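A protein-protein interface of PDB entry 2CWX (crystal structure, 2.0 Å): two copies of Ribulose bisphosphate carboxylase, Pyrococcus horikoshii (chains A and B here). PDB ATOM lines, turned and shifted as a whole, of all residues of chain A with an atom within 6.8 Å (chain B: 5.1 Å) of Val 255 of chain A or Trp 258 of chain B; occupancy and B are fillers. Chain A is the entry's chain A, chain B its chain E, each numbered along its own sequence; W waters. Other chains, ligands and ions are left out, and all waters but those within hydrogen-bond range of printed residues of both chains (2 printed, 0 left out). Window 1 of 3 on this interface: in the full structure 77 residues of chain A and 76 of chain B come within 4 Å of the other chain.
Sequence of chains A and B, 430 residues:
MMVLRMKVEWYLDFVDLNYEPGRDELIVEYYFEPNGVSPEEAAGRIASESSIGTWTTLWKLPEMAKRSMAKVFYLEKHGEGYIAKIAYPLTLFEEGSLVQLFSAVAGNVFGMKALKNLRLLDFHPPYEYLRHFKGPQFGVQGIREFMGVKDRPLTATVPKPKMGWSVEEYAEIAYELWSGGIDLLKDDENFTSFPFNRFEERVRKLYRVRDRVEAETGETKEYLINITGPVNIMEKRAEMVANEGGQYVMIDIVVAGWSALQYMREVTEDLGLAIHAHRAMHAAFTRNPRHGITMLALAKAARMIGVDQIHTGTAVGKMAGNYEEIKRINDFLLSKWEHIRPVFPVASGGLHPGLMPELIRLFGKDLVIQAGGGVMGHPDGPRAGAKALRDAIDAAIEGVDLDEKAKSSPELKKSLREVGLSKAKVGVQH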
ATOM      1  N   THR A 228       5.609  -4.492  33.240  1.00  0.00           N
ATOM      2  CA  THR A 228       5.098  -5.078  31.996  1.00  0.00           C
ATOM      3  C   THR A 228       5.510  -6.532  31.877  1.00  0.00           C
ATOM      4  O   THR A 228       6.648  -6.850  32.115  1.00  0.00           O
ATOM      5  CB  THR A 228       5.693  -4.317  30.775  1.00  0.00           C
ATOM      6  OG1 THR A 228       5.358  -2.928  30.849  1.00  0.00           O
ATOM      7  CG2 THR A 228       5.081  -4.765  29.490  1.00  0.00           C
ATOM      8  N   GLY A 229       4.567  -7.388  31.494  1.00  0.00           N
ATOM      9  CA  GLY A 229       4.797  -8.812  31.261  1.00  0.00           C
ATOM     10  C   GLY A 229       3.480  -9.518  30.948  1.00  0.00           C
ATOM     11  O   GLY A 229       2.442  -8.859  30.844  1.00  0.00           O
ATOM     12  N   PRO A 230       3.499 -10.840  30.809  1.00  0.00           N
ATOM     13  CA  PRO A 230       2.254 -11.623  30.828  1.00  0.00           C
ATOM     14  C   PRO A 230       1.430 -11.227  32.056  1.00  0.00           C
ATOM     15  O   PRO A 230       2.019 -10.928  33.103  1.00  0.00           O
ATOM     16  CB  PRO A 230       2.739 -13.054  30.953  1.00  0.00           C
ATOM     17  CG  PRO A 230       4.130 -13.018  30.399  1.00  0.00           C
ATOM     18  CD  PRO A 230       4.690 -11.693  30.752  1.00  0.00           C
ATOM     19  N   VAL A 231       0.099 -11.201  31.944  1.00  0.00           N
ATOM     20  CA  VAL A 231      -0.680 -10.534  32.956  1.00  0.00           C
ATOM     21  C   VAL A 231      -0.491 -11.045  34.337  1.00  0.00           C
ATOM     22  O   VAL A 231      -0.586 -10.274  35.249  1.00  0.00           O
ATOM     23  CB  VAL A 231      -2.220 -10.616  32.852  1.00  0.00           C
ATOM     24  CG1 VAL A 231      -2.811  -9.242  33.170  1.00  0.00           C
ATOM     25  CG2 VAL A 231      -2.687 -11.179  31.646  1.00  0.00           C
ATOM     26  N   ASP A 252       3.635  -0.809  29.774  1.00  0.00           N
ATOM     27  CA  ASP A 252       3.773  -0.494  28.360  1.00  0.00           C
ATOM     28  C   ASP A 252       2.434  -0.934  27.761  1.00  0.00           C
ATOM     29  O   ASP A 252       2.258  -2.098  27.419  1.00  0.00           O
ATOM     30  CB  ASP A 252       4.875  -1.303  27.684  1.00  0.00           C
ATOM     31  CG  ASP A 252       6.276  -1.067  28.253  1.00  0.00           C
ATOM     32  OD1 ASP A 252       6.487  -0.059  28.919  1.00  0.00           O
ATOM     33  OD2 ASP A 252       7.251  -1.872  28.043  1.00  0.00           O
ATOM     34  N   ILE A 253       1.483  -0.023  27.674  1.00  0.00           N
ATOM     35  CA  ILE A 253       0.093  -0.415  27.426  1.00  0.00           C
ATOM     36  C   ILE A 253      -0.182  -0.851  25.999  1.00  0.00           C
ATOM     37  O   ILE A 253      -1.104  -1.604  25.779  1.00  0.00           O
ATOM     38  CB  ILE A 253      -0.903   0.720  27.819  1.00  0.00           C
ATOM     39  CG1 ILE A 253      -0.705   1.941  26.946  1.00  0.00           C
ATOM     40  CG2 ILE A 253      -0.724   1.098  29.307  1.00  0.00           C
ATOM     41  CD1 ILE A 253      -1.876   2.851  26.859  1.00  0.00           C
ATOM     42  N   VAL A 254       0.629  -0.420  25.041  1.00  0.00           N
ATOM     43  CA  VAL A 254       0.445  -0.837  23.657  1.00  0.00           C
ATOM     44  C   VAL A 254       0.958  -2.266  23.472  1.00  0.00           C
ATOM     45  O   VAL A 254       0.276  -3.110  22.958  1.00  0.00           O
ATOM     46  CB  VAL A 254       1.042   0.165  22.622  1.00  0.00           C
ATOM     47  CG1 VAL A 254       0.793  -0.347  21.245  1.00  0.00           C
ATOM     48  CG2 VAL A 254       0.359   1.507  22.739  1.00  0.00           C
ATOM     49  N   VAL A 255       2.136  -2.545  23.968  1.00  0.00           N
ATOM     50  CA  VAL A 255       2.678  -3.883  23.859  1.00  0.00           C
ATOM     51  C   VAL A 255       1.868  -4.869  24.671  1.00  0.00           C
ATOM     52  O   VAL A 255       1.596  -5.953  24.232  1.00  0.00           O
ATOM     53  CB  VAL A 255       4.141  -3.926  24.366  1.00  0.00           C
ATOM     54  CG1 VAL A 255       4.738  -5.255  24.008  1.00  0.00           C
ATOM     55  CG2 VAL A 255       4.942  -2.812  23.688  1.00  0.00           C
ATOM     56  N   ALA A 256       1.456  -4.471  25.864  1.00  0.00           N
ATOM     57  CA  ALA A 256       0.687  -5.347  26.741  1.00  0.00           C
ATOM     58  C   ALA A 256      -0.736  -5.578  26.283  1.00  0.00           C
ATOM     59  O   ALA A 256      -1.221  -6.724  26.286  1.00  0.00           O
ATOM     60  CB  ALA A 256       0.689  -4.793  28.158  1.00  0.00           C
ATOM     61  N   GLY A 257      -1.425  -4.495  25.897  1.00  0.00           N
ATOM     62  CA  GLY A 257      -2.728  -4.598  25.299  1.00  0.00           C
ATOM     63  C   GLY A 257      -3.908  -4.285  26.219  1.00  0.00           C
ATOM     64  O   GLY A 257      -3.798  -4.222  27.447  1.00  0.00           O
ATOM     65  N   TRP A 258      -5.042  -4.040  25.578  1.00  0.00           N
ATOM     66  CA  TRP A 258      -6.222  -3.528  26.244  1.00  0.00           C
ATOM     67  C   TRP A 258      -6.809  -4.535  27.238  1.00  0.00           C
ATOM     68  O   TRP A 258      -7.335  -4.121  28.220  1.00  0.00           O
ATOM     69  CB  TRP A 258      -7.304  -3.148  25.235  1.00  0.00           C
ATOM     70  CG  TRP A 258      -6.918  -2.100  24.311  1.00  0.00           C
ATOM     71  CD1 TRP A 258      -6.818  -2.210  22.962  1.00  0.00           C
ATOM     72  CD2 TRP A 258      -6.569  -0.746  24.627  1.00  0.00           C
ATOM     73  NE1 TRP A 258      -6.413  -1.018  22.425  1.00  0.00           N
ATOM     74  CE2 TRP A 258      -6.275  -0.100  23.422  1.00  0.00           C
ATOM     75  CE3 TRP A 258      -6.510  -0.010  25.803  1.00  0.00           C
ATOM     76  CZ2 TRP A 258      -5.882   1.229  23.358  1.00  0.00           C
ATOM     77  CZ3 TRP A 258      -6.119   1.318  25.736  1.00  0.00           C
ATOM     78  CH2 TRP A 258      -5.817   1.915  24.536  1.00  0.00           C
ATOM     79  N   ALA A 260      -5.333  -6.822  29.093  1.00  0.00           N
ATOM     80  CA  ALA A 260      -4.522  -6.840  30.297  1.00  0.00           C
ATOM     81  C   ALA A 260      -4.675  -5.526  31.029  1.00  0.00           C
ATOM     82  O   ALA A 260      -4.781  -5.510  32.251  1.00  0.00           O
ATOM     83  CB  ALA A 260      -3.067  -7.076  29.955  1.00  0.00           C
ATOM     84  N   HIS A 278       3.337   3.888  29.337  1.00  0.00           N
ATOM     85  CA  HIS A 278       4.288   4.060  28.264  1.00  0.00           C
ATOM     86  C   HIS A 278       3.624   3.599  26.968  1.00  0.00           C
ATOM     87  O   HIS A 278       2.912   2.601  26.940  1.00  0.00           O
ATOM     88  CB  HIS A 278       5.493   3.167  28.482  1.00  0.00           C
ATOM     89  CG  HIS A 278       6.721   3.642  27.777  1.00  0.00           C
ATOM     90  ND1 HIS A 278       6.863   3.584  26.410  1.00  0.00           N
ATOM     91  CD2 HIS A 278       7.892   4.142  28.262  1.00  0.00           C
ATOM     92  CE1 HIS A 278       8.052   4.066  26.072  1.00  0.00           C
ATOM     93  NE2 HIS A 278       8.696   4.410  27.180  1.00  0.00           N
ATOM     94  N   ARG A 279       3.873   4.316  25.900  1.00  0.00           N
ATOM     95  CA  ARG A 279       3.133   4.060  24.690  1.00  0.00           C
ATOM     96  C   ARG A 279       3.990   3.384  23.608  1.00  0.00           C
ATOM     97  O   ARG A 279       3.618   3.415  22.443  1.00  0.00           O
ATOM     98  CB  ARG A 279       2.539   5.371  24.179  1.00  0.00           C
ATOM     99  CG  ARG A 279       3.581   6.379  23.711  1.00  0.00           C
ATOM    100  CD  ARG A 279       2.940   7.624  23.025  1.00  0.00           C
ATOM    101  NE  ARG A 279       3.974   8.535  22.545  1.00  0.00           N
ATOM    102  CZ  ARG A 279       3.755   9.588  21.769  1.00  0.00           C
ATOM    103  NH1 ARG A 279       2.524   9.889  21.392  1.00  0.00           N
ATOM    104  NH2 ARG A 279       4.776  10.338  21.362  1.00  0.00           N
ATOM    105  N   ALA A 280       5.075   2.718  23.995  1.00  0.00           N
ATOM    106  CA  ALA A 280       5.943   2.015  23.027  1.00  0.00           C
ATOM    107  C   ALA A 280       5.153   1.111  22.053  1.00  0.00           C
ATOM    108  O   ALA A 280       4.244   0.377  22.479  1.00  0.00           O
ATOM    109  CB  ALA A 280       7.066   1.185  23.792  1.00  0.00           C
ATOM    110  N   MET A 281       5.508   1.186  20.763  1.00  0.00           N
ATOM    111  CA  MET A 281       4.855   0.488  19.643  1.00  0.00           C
ATOM    112  C   MET A 281       3.692   1.289  19.035  1.00  0.00           C
ATOM    113  O   MET A 281       3.252   0.969  17.919  1.00  0.00           O
ATOM    114  CB  MET A 281       4.393  -0.932  20.008  1.00  0.00           C
ATOM    115  CG  MET A 281       4.125  -1.893  18.823  1.00  0.00           C
ATOM    116  SD  MET A 281       3.652  -3.639  19.405  1.00  0.00           S
ATOM    117  CE  MET A 281       2.125  -3.334  19.911  1.00  0.00           C
ATOM    118  N   HIS A 282       3.224   2.336  19.735  1.00  0.00           N
ATOM    119  CA  HIS A 282       2.089   3.154  19.253  1.00  0.00           C
ATOM    120  C   HIS A 282       2.294   3.616  17.805  1.00  0.00           C
ATOM    121  O   HIS A 282       1.348   3.598  17.011  1.00  0.00           O
ATOM    122  CB  HIS A 282       1.810   4.400  20.150  1.00  0.00           C
ATOM    123  CG  HIS A 282       2.788   5.526  19.952  1.00  0.00           C
ATOM    124  ND1 HIS A 282       2.533   6.594  19.111  1.00  0.00           N
ATOM    125  CD2 HIS A 282       4.032   5.732  20.451  1.00  0.00           C
ATOM    126  CE1 HIS A 282       3.577   7.413  19.119  1.00  0.00           C
ATOM    127  NE2 HIS A 282       4.496   6.915  19.929  1.00  0.00           N
ATOM    128  N   LEU B  98       7.223 -12.682  25.639  1.00  0.00           N
ATOM    129  CA  LEU B  98       7.112 -12.143  24.281  1.00  0.00           C
ATOM    130  C   LEU B  98       6.762 -10.671  24.383  1.00  0.00           C
ATOM    131  O   LEU B  98       7.197  -9.864  23.577  1.00  0.00           O
ATOM    132  CB  LEU B  98       6.069 -12.938  23.526  1.00  0.00           C
ATOM    133  CG  LEU B  98       5.732 -12.609  22.079  1.00  0.00           C
ATOM    134  CD1 LEU B  98       4.811 -11.344  22.013  1.00  0.00           C
ATOM    135  CD2 LEU B  98       6.944 -12.473  21.231  1.00  0.00           C
ATOM    136  N   VAL B  99       6.041 -10.298  25.436  1.00  0.00           N
ATOM    137  CA  VAL B  99       5.738  -8.913  25.671  1.00  0.00           C
ATOM    138  C   VAL B  99       6.986  -8.060  25.712  1.00  0.00           C
ATOM    139  O   VAL B  99       7.052  -7.023  25.074  1.00  0.00           O
ATOM    140  CB  VAL B  99       4.904  -8.709  26.986  1.00  0.00           C
ATOM    141  CG1 VAL B  99       4.510  -7.281  27.111  1.00  0.00           C
ATOM    142  CG2 VAL B  99       3.643  -9.554  26.926  1.00  0.00           C
ATOM    143  N   PHE B 102       8.799  -7.759  22.242  1.00  0.00           N
ATOM    144  CA  PHE B 102       8.138  -6.751  21.403  1.00  0.00           C
ATOM    145  C   PHE B 102       8.352  -5.312  21.914  1.00  0.00           C
ATOM    146  O   PHE B 102       8.505  -4.394  21.097  1.00  0.00           O
ATOM    147  CB  PHE B 102       6.659  -7.093  21.136  1.00  0.00           C
ATOM    148  CG  PHE B 102       6.455  -8.034  19.948  1.00  0.00           C
ATOM    149  CD1 PHE B 102       7.328  -9.075  19.704  1.00  0.00           C
ATOM    150  CD2 PHE B 102       5.439  -7.818  19.034  1.00  0.00           C
ATOM    151  CE1 PHE B 102       7.179  -9.905  18.588  1.00  0.00           C
ATOM    152  CE2 PHE B 102       5.261  -8.654  17.929  1.00  0.00           C
ATOM    153  CZ  PHE B 102       6.147  -9.695  17.699  1.00  0.00           C
ATOM    154  N   SER B 103       8.501  -5.102  23.224  1.00  0.00           N
ATOM    155  CA  SER B 103       8.823  -3.754  23.704  1.00  0.00           C
ATOM    156  C   SER B 103      10.212  -3.337  23.248  1.00  0.00           C
ATOM    157  O   SER B 103      10.429  -2.186  22.943  1.00  0.00           O
ATOM    158  CB  SER B 103       8.749  -3.621  25.220  1.00  0.00           C
ATOM    159  OG  SER B 103       9.821  -4.366  25.834  1.00  0.00           O
ATOM    160  N   ILE B 253      -6.879 -11.779  19.076  1.00  0.00           N
ATOM    161  CA  ILE B 253      -5.577 -11.599  19.745  1.00  0.00           C
ATOM    162  C   ILE B 253      -4.938 -10.220  19.647  1.00  0.00           C
ATOM    163  O   ILE B 253      -4.172  -9.843  20.515  1.00  0.00           O
ATOM    164  CB  ILE B 253      -4.559 -12.673  19.322  1.00  0.00           C
ATOM    165  CG1 ILE B 253      -4.287 -12.665  17.813  1.00  0.00           C
ATOM    166  CG2 ILE B 253      -5.040 -14.055  19.728  1.00  0.00           C
ATOM    167  CD1 ILE B 253      -2.967 -13.356  17.459  1.00  0.00           C
ATOM    168  N   ALA B 256      -7.070  -7.955  22.037  1.00  0.00           N
ATOM    169  CA  ALA B 256      -6.849  -8.345  23.413  1.00  0.00           C
ATOM    170  C   ALA B 256      -5.411  -7.993  23.829  1.00  0.00           C
ATOM    171  O   ALA B 256      -5.173  -7.391  24.882  1.00  0.00           O
ATOM    172  CB  ALA B 256      -7.124  -9.837  23.600  1.00  0.00           C
ATOM    173  N   GLY B 257      -4.459  -8.434  23.013  1.00  0.00           N
ATOM    174  CA  GLY B 257      -3.044  -8.079  23.170  1.00  0.00           C
ATOM    175  C   GLY B 257      -2.223  -9.244  23.752  1.00  0.00           C
ATOM    176  O   GLY B 257      -2.777 -10.234  24.293  1.00  0.00           O
ATOM    177  N   TRP B 258      -0.909  -9.066  23.700  1.00  0.00           N
ATOM    178  CA  TRP B 258       0.058 -10.125  23.934  1.00  0.00           C
ATOM    179  C   TRP B 258       0.144 -10.533  25.377  1.00  0.00           C
ATOM    180  O   TRP B 258       0.329 -11.697  25.666  1.00  0.00           O
ATOM    181  CB  TRP B 258       1.469  -9.683  23.479  1.00  0.00           C
ATOM    182  CG  TRP B 258       1.625  -9.472  21.992  1.00  0.00           C
ATOM    183  CD1 TRP B 258       2.049  -8.317  21.390  1.00  0.00           C
ATOM    184  CD2 TRP B 258       1.438 -10.415  20.938  1.00  0.00           C
ATOM    185  NE1 TRP B 258       2.064  -8.467  20.023  1.00  0.00           N
ATOM    186  CE2 TRP B 258       1.715  -9.751  19.716  1.00  0.00           C
ATOM    187  CE3 TRP B 258       1.070 -11.749  20.885  1.00  0.00           C
ATOM    188  CZ2 TRP B 258       1.610 -10.374  18.468  1.00  0.00           C
ATOM    189  CZ3 TRP B 258       0.987 -12.368  19.654  1.00  0.00           C
ATOM    190  CH2 TRP B 258       1.246 -11.677  18.460  1.00  0.00           C
ATOM    191  N   SER B 259       0.025  -9.581  26.293  1.00  0.00           N
ATOM    192  CA  SER B 259       0.036  -9.900  27.729  1.00  0.00           C
ATOM    193  C   SER B 259      -1.106 -10.839  28.135  1.00  0.00           C
ATOM    194  O   SER B 259      -0.922 -11.822  28.872  1.00  0.00           O
ATOM    195  CB  SER B 259      -0.042  -8.612  28.518  1.00  0.00           C
ATOM    196  OG  SER B 259      -0.066  -8.843  29.910  1.00  0.00           O
ATOM    197  N   ALA B 260      -2.310 -10.526  27.692  1.00  0.00           N
ATOM    198  CA  ALA B 260      -3.429 -11.411  27.933  1.00  0.00           C
ATOM    199  C   ALA B 260      -3.279 -12.746  27.225  1.00  0.00           C
ATOM    200  O   ALA B 260      -3.654 -13.780  27.780  1.00  0.00           O
ATOM    201  CB  ALA B 260      -4.691 -10.783  27.496  1.00  0.00           C
ATOM    202  N   LEU B 261      -2.779 -12.741  25.993  1.00  0.00           N
ATOM    203  CA  LEU B 261      -2.634 -13.994  25.254  1.00  0.00           C
ATOM    204  C   LEU B 261      -1.669 -14.977  25.918  1.00  0.00           C
ATOM    205  O   LEU B 261      -1.945 -16.183  25.953  1.00  0.00           O
ATOM    206  CB  LEU B 261      -2.085 -13.746  23.864  1.00  0.00           C
ATOM    207  CG  LEU B 261      -2.484 -14.642  22.712  1.00  0.00           C
ATOM    208  CD1 LEU B 261      -1.409 -14.823  21.657  1.00  0.00           C
ATOM    209  CD2 LEU B 261      -3.209 -15.882  22.983  1.00  0.00           C
ATOM    210  N   GLN B 262      -0.533 -14.474  26.370  1.00  0.00           N
ATOM    211  CA  GLN B 262       0.439 -15.332  27.056  1.00  0.00           C
ATOM    212  C   GLN B 262      -0.196 -15.977  28.291  1.00  0.00           C
ATOM    213  O   GLN B 262      -0.043 -17.157  28.537  1.00  0.00           O
ATOM    214  CB  GLN B 262       1.716 -14.591  27.423  1.00  0.00           C
ATOM    215  CG  GLN B 262       2.598 -14.196  26.248  1.00  0.00           C
ATOM    216  CD  GLN B 262       4.065 -14.021  26.652  1.00  0.00           C
ATOM    217  OE1 GLN B 262       4.568 -12.908  26.652  1.00  0.00           O
ATOM    218  NE2 GLN B 262       4.715 -15.105  27.090  1.00  0.00           N
ATOM    219  N   TYR B 263      -0.951 -15.197  29.044  1.00  0.00           N
ATOM    220  CA  TYR B 263      -1.600 -15.723  30.210  1.00  0.00           C
ATOM    221  C   TYR B 263      -2.689 -16.738  29.831  1.00  0.00           C
ATOM    222  O   TYR B 263      -2.793 -17.781  30.446  1.00  0.00           O
ATOM    223  CB  TYR B 263      -2.196 -14.615  31.049  1.00  0.00           C
ATOM    224  CG  TYR B 263      -2.991 -15.145  32.200  1.00  0.00           C
ATOM    225  CD1 TYR B 263      -2.364 -15.812  33.244  1.00  0.00           C
ATOM    226  CD2 TYR B 263      -4.366 -15.034  32.218  1.00  0.00           C
ATOM    227  CE1 TYR B 263      -3.077 -16.333  34.324  1.00  0.00           C
ATOM    228  CE2 TYR B 263      -5.091 -15.580  33.264  1.00  0.00           C
ATOM    229  CZ  TYR B 263      -4.432 -16.220  34.313  1.00  0.00           C
ATOM    230  OH  TYR B 263      -5.148 -16.733  35.343  1.00  0.00           O
ATOM    231  N   LEU B 298       3.714 -11.273  13.037  1.00  0.00           N
ATOM    232  CA  LEU B 298       2.599 -11.476  13.935  1.00  0.00           C
ATOM    233  C   LEU B 298       2.305 -12.965  14.065  1.00  0.00           C
ATOM    234  O   LEU B 298       2.180 -13.485  15.177  1.00  0.00           O
ATOM    235  CB  LEU B 298       1.397 -10.762  13.383  1.00  0.00           C
ATOM    236  CG  LEU B 298       0.342 -10.268  14.332  1.00  0.00           C
ATOM    237  CD1 LEU B 298      -0.452  -9.133  13.612  1.00  0.00           C
ATOM    238  CD2 LEU B 298      -0.579 -11.413  14.710  1.00  0.00           C
ATOM    239  N   ALA B 301       4.938 -14.785  16.194  1.00  0.00           N
ATOM    240  CA  ALA B 301       4.712 -14.601  17.628  1.00  0.00           C
ATOM    241  C   ALA B 301       3.507 -15.393  18.158  1.00  0.00           C
ATOM    242  O   ALA B 301       3.565 -15.997  19.228  1.00  0.00           O
ATOM    243  CB  ALA B 301       4.532 -13.159  17.939  1.00  0.00           C
ATOM    244  N   ALA B 302       2.408 -15.326  17.435  1.00  0.00           N
ATOM    245  CA  ALA B 302       1.216 -16.098  17.800  1.00  0.00           C
ATOM    246  C   ALA B 302       1.452 -17.613  17.838  1.00  0.00           C
ATOM    247  O   ALA B 302       1.009 -18.272  18.766  1.00  0.00           O
ATOM    248  CB  ALA B 302       0.057 -15.763  16.833  1.00  0.00           C
ATOM    249  N   ILE B 305       3.763 -18.524  20.994  1.00  0.00           N
ATOM    250  CA  ILE B 305       2.984 -18.576  22.239  1.00  0.00           C
ATOM    251  C   ILE B 305       2.075 -19.831  22.212  1.00  0.00           C
ATOM    252  O   ILE B 305       2.017 -20.633  23.165  1.00  0.00           O
ATOM    253  CB  ILE B 305       2.177 -17.291  22.406  1.00  0.00           C
ATOM    254  CG1 ILE B 305       3.094 -16.147  22.741  1.00  0.00           C
ATOM    255  CG2 ILE B 305       1.124 -17.432  23.516  1.00  0.00           C
ATOM    256  CD1 ILE B 305       2.447 -14.750  22.530  1.00  0.00           C
HETATM  257  O   HOH W   1      -3.572  -7.762  26.902  1.00  0.00           O
HETATM  258  O   HOH W   2      -0.646  -6.364  22.397  1.00  0.00           O
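The backbone NH (N) of Val 231 of chain A lies within hydrogen-bond range of the side-chain hydroxyl (OG) of Ser 259 of chain B (3.1 Å). The backbone NH (N) of Trp 258 of chain A lies within hydrogen-bond range of the backbone carbonyl oxygen (O) of Ala 256 of chain B. OG of Ser 259 of chain B sits at hydrogen-bond distance from O of Gly 229 of chain A, 2.7 Å away. O of Ala 256 of chain A lies within hydrogen-bond range of N of Ser 259 of chain B, at 3.1 Å.
Val 255 of chain A touches just these residues of chain B: Val 99, Phe 102, Ser 103 and Trp 258. Trp 258 of chain B touches just these residues of chain A: Val 255 (3.7 Å) and Ala 256 (3.5 Å). Printed residues of chain B within 4 Å of Pro 230 of chain A: Ser 259 (3.5 Å) and Gln 262 (3.8 Å). Printed residues of chain A within 4 Å of Ser 259 of chain B: Gly 229 (2.7 Å), Pro 230 (3.5 Å), Val 231 (3.1 Å), Ala 256 (3.1 Å) and Ala 260 (3.5 Å). Ile 253 of chain A touches none of the printed residues of chain B.
Thr 228 of chain A touches Val 99 of chain B. Ser 259 of chain B touches Pro 230 of chain A (OG to C, 3.5 Å). CG2 of Val 231 of chain A touches CA of Ala 260 of chain B, at 3.8 Å. Val 231 of chain A touches Tyr 263 of chain B (CG2 to CB, 3.5 Å). Asp 252 of chain A touches Ser 103 of chain B. Val 255 of chain A touches Trp 258 of chain B. Ala 256 of chain A touches Gly 257 of chain B (O to C, 3.7 Å). Ala 256 of chain A touches Trp 258 of chain B (O to N, 3.5 Å). Gly 257 of chain A touches Ala 256 of chain B. OG of Ser 259 of chain B touches CB of Ala 260 of chain A (3.5 Å).
The side-chain amide oxygen of Gln 262 of chain B sits at hydrogen-bond distance from the backbone NH of Leu 98 of chain B. The backbone NH (N) of Val 99 of chain B sits at hydrogen-bond distance from the side-chain amide oxygen (OE1) of Gln 262 of chain B, 3.2 Å away. The side-chain hydroxyl of Thr 228 of chain A sits at hydrogen-bond distance from the backbone NH of Asp 252 of chain A, at 2.9 Å.
Ala 256 of chain A touches Gly 257 of chain B, and with the chains exchanged Gly 257 of chain A touches Ala 256 of chain B. Ala 256 of chain A touches Trp 258 of chain B, and with the chains exchanged Trp 258 of chain A touches Ala 256 of chain B. 5 positions are printed for both chains.
Of the 17 printed residues of chain A, 10 touch a printed residue of chain B. Printed residues of chain A that touch a printed residue of chain B: Thr 228, Gly 229, Pro 230, Val 231, Asp 252, Val 255, Ala 256, Gly 257, Trp 258 and Ala 260. Printed residues of chain B that touch a printed residue of chain A: Val 99, Phe 102, Ser 103, Ala 256, Gly 257, Trp 258, Ser 259, Ala 260, Gln 262 and Tyr 263. Among the printed residues, no Asp or Glu carboxylate lies within 4 Å of a Lys or Arg side-chain nitrogen of the other chain.
Water W1 lies within hydrogen-bond range of the backbone carbonyl oxygen of Ala 256 of chain B, the backbone carbonyl oxygen of Ala 256 of chain A, the backbone NH of Ala 260 of chain A and the backbone NH of Ala 260 of chain B. Water W2 lies within hydrogen-bond range of O of Val 255 of chain A (2.9 Å), N of Trp 258 of chain B (3.0 Å) and O of Val 254 of chain A (3.4 Å).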
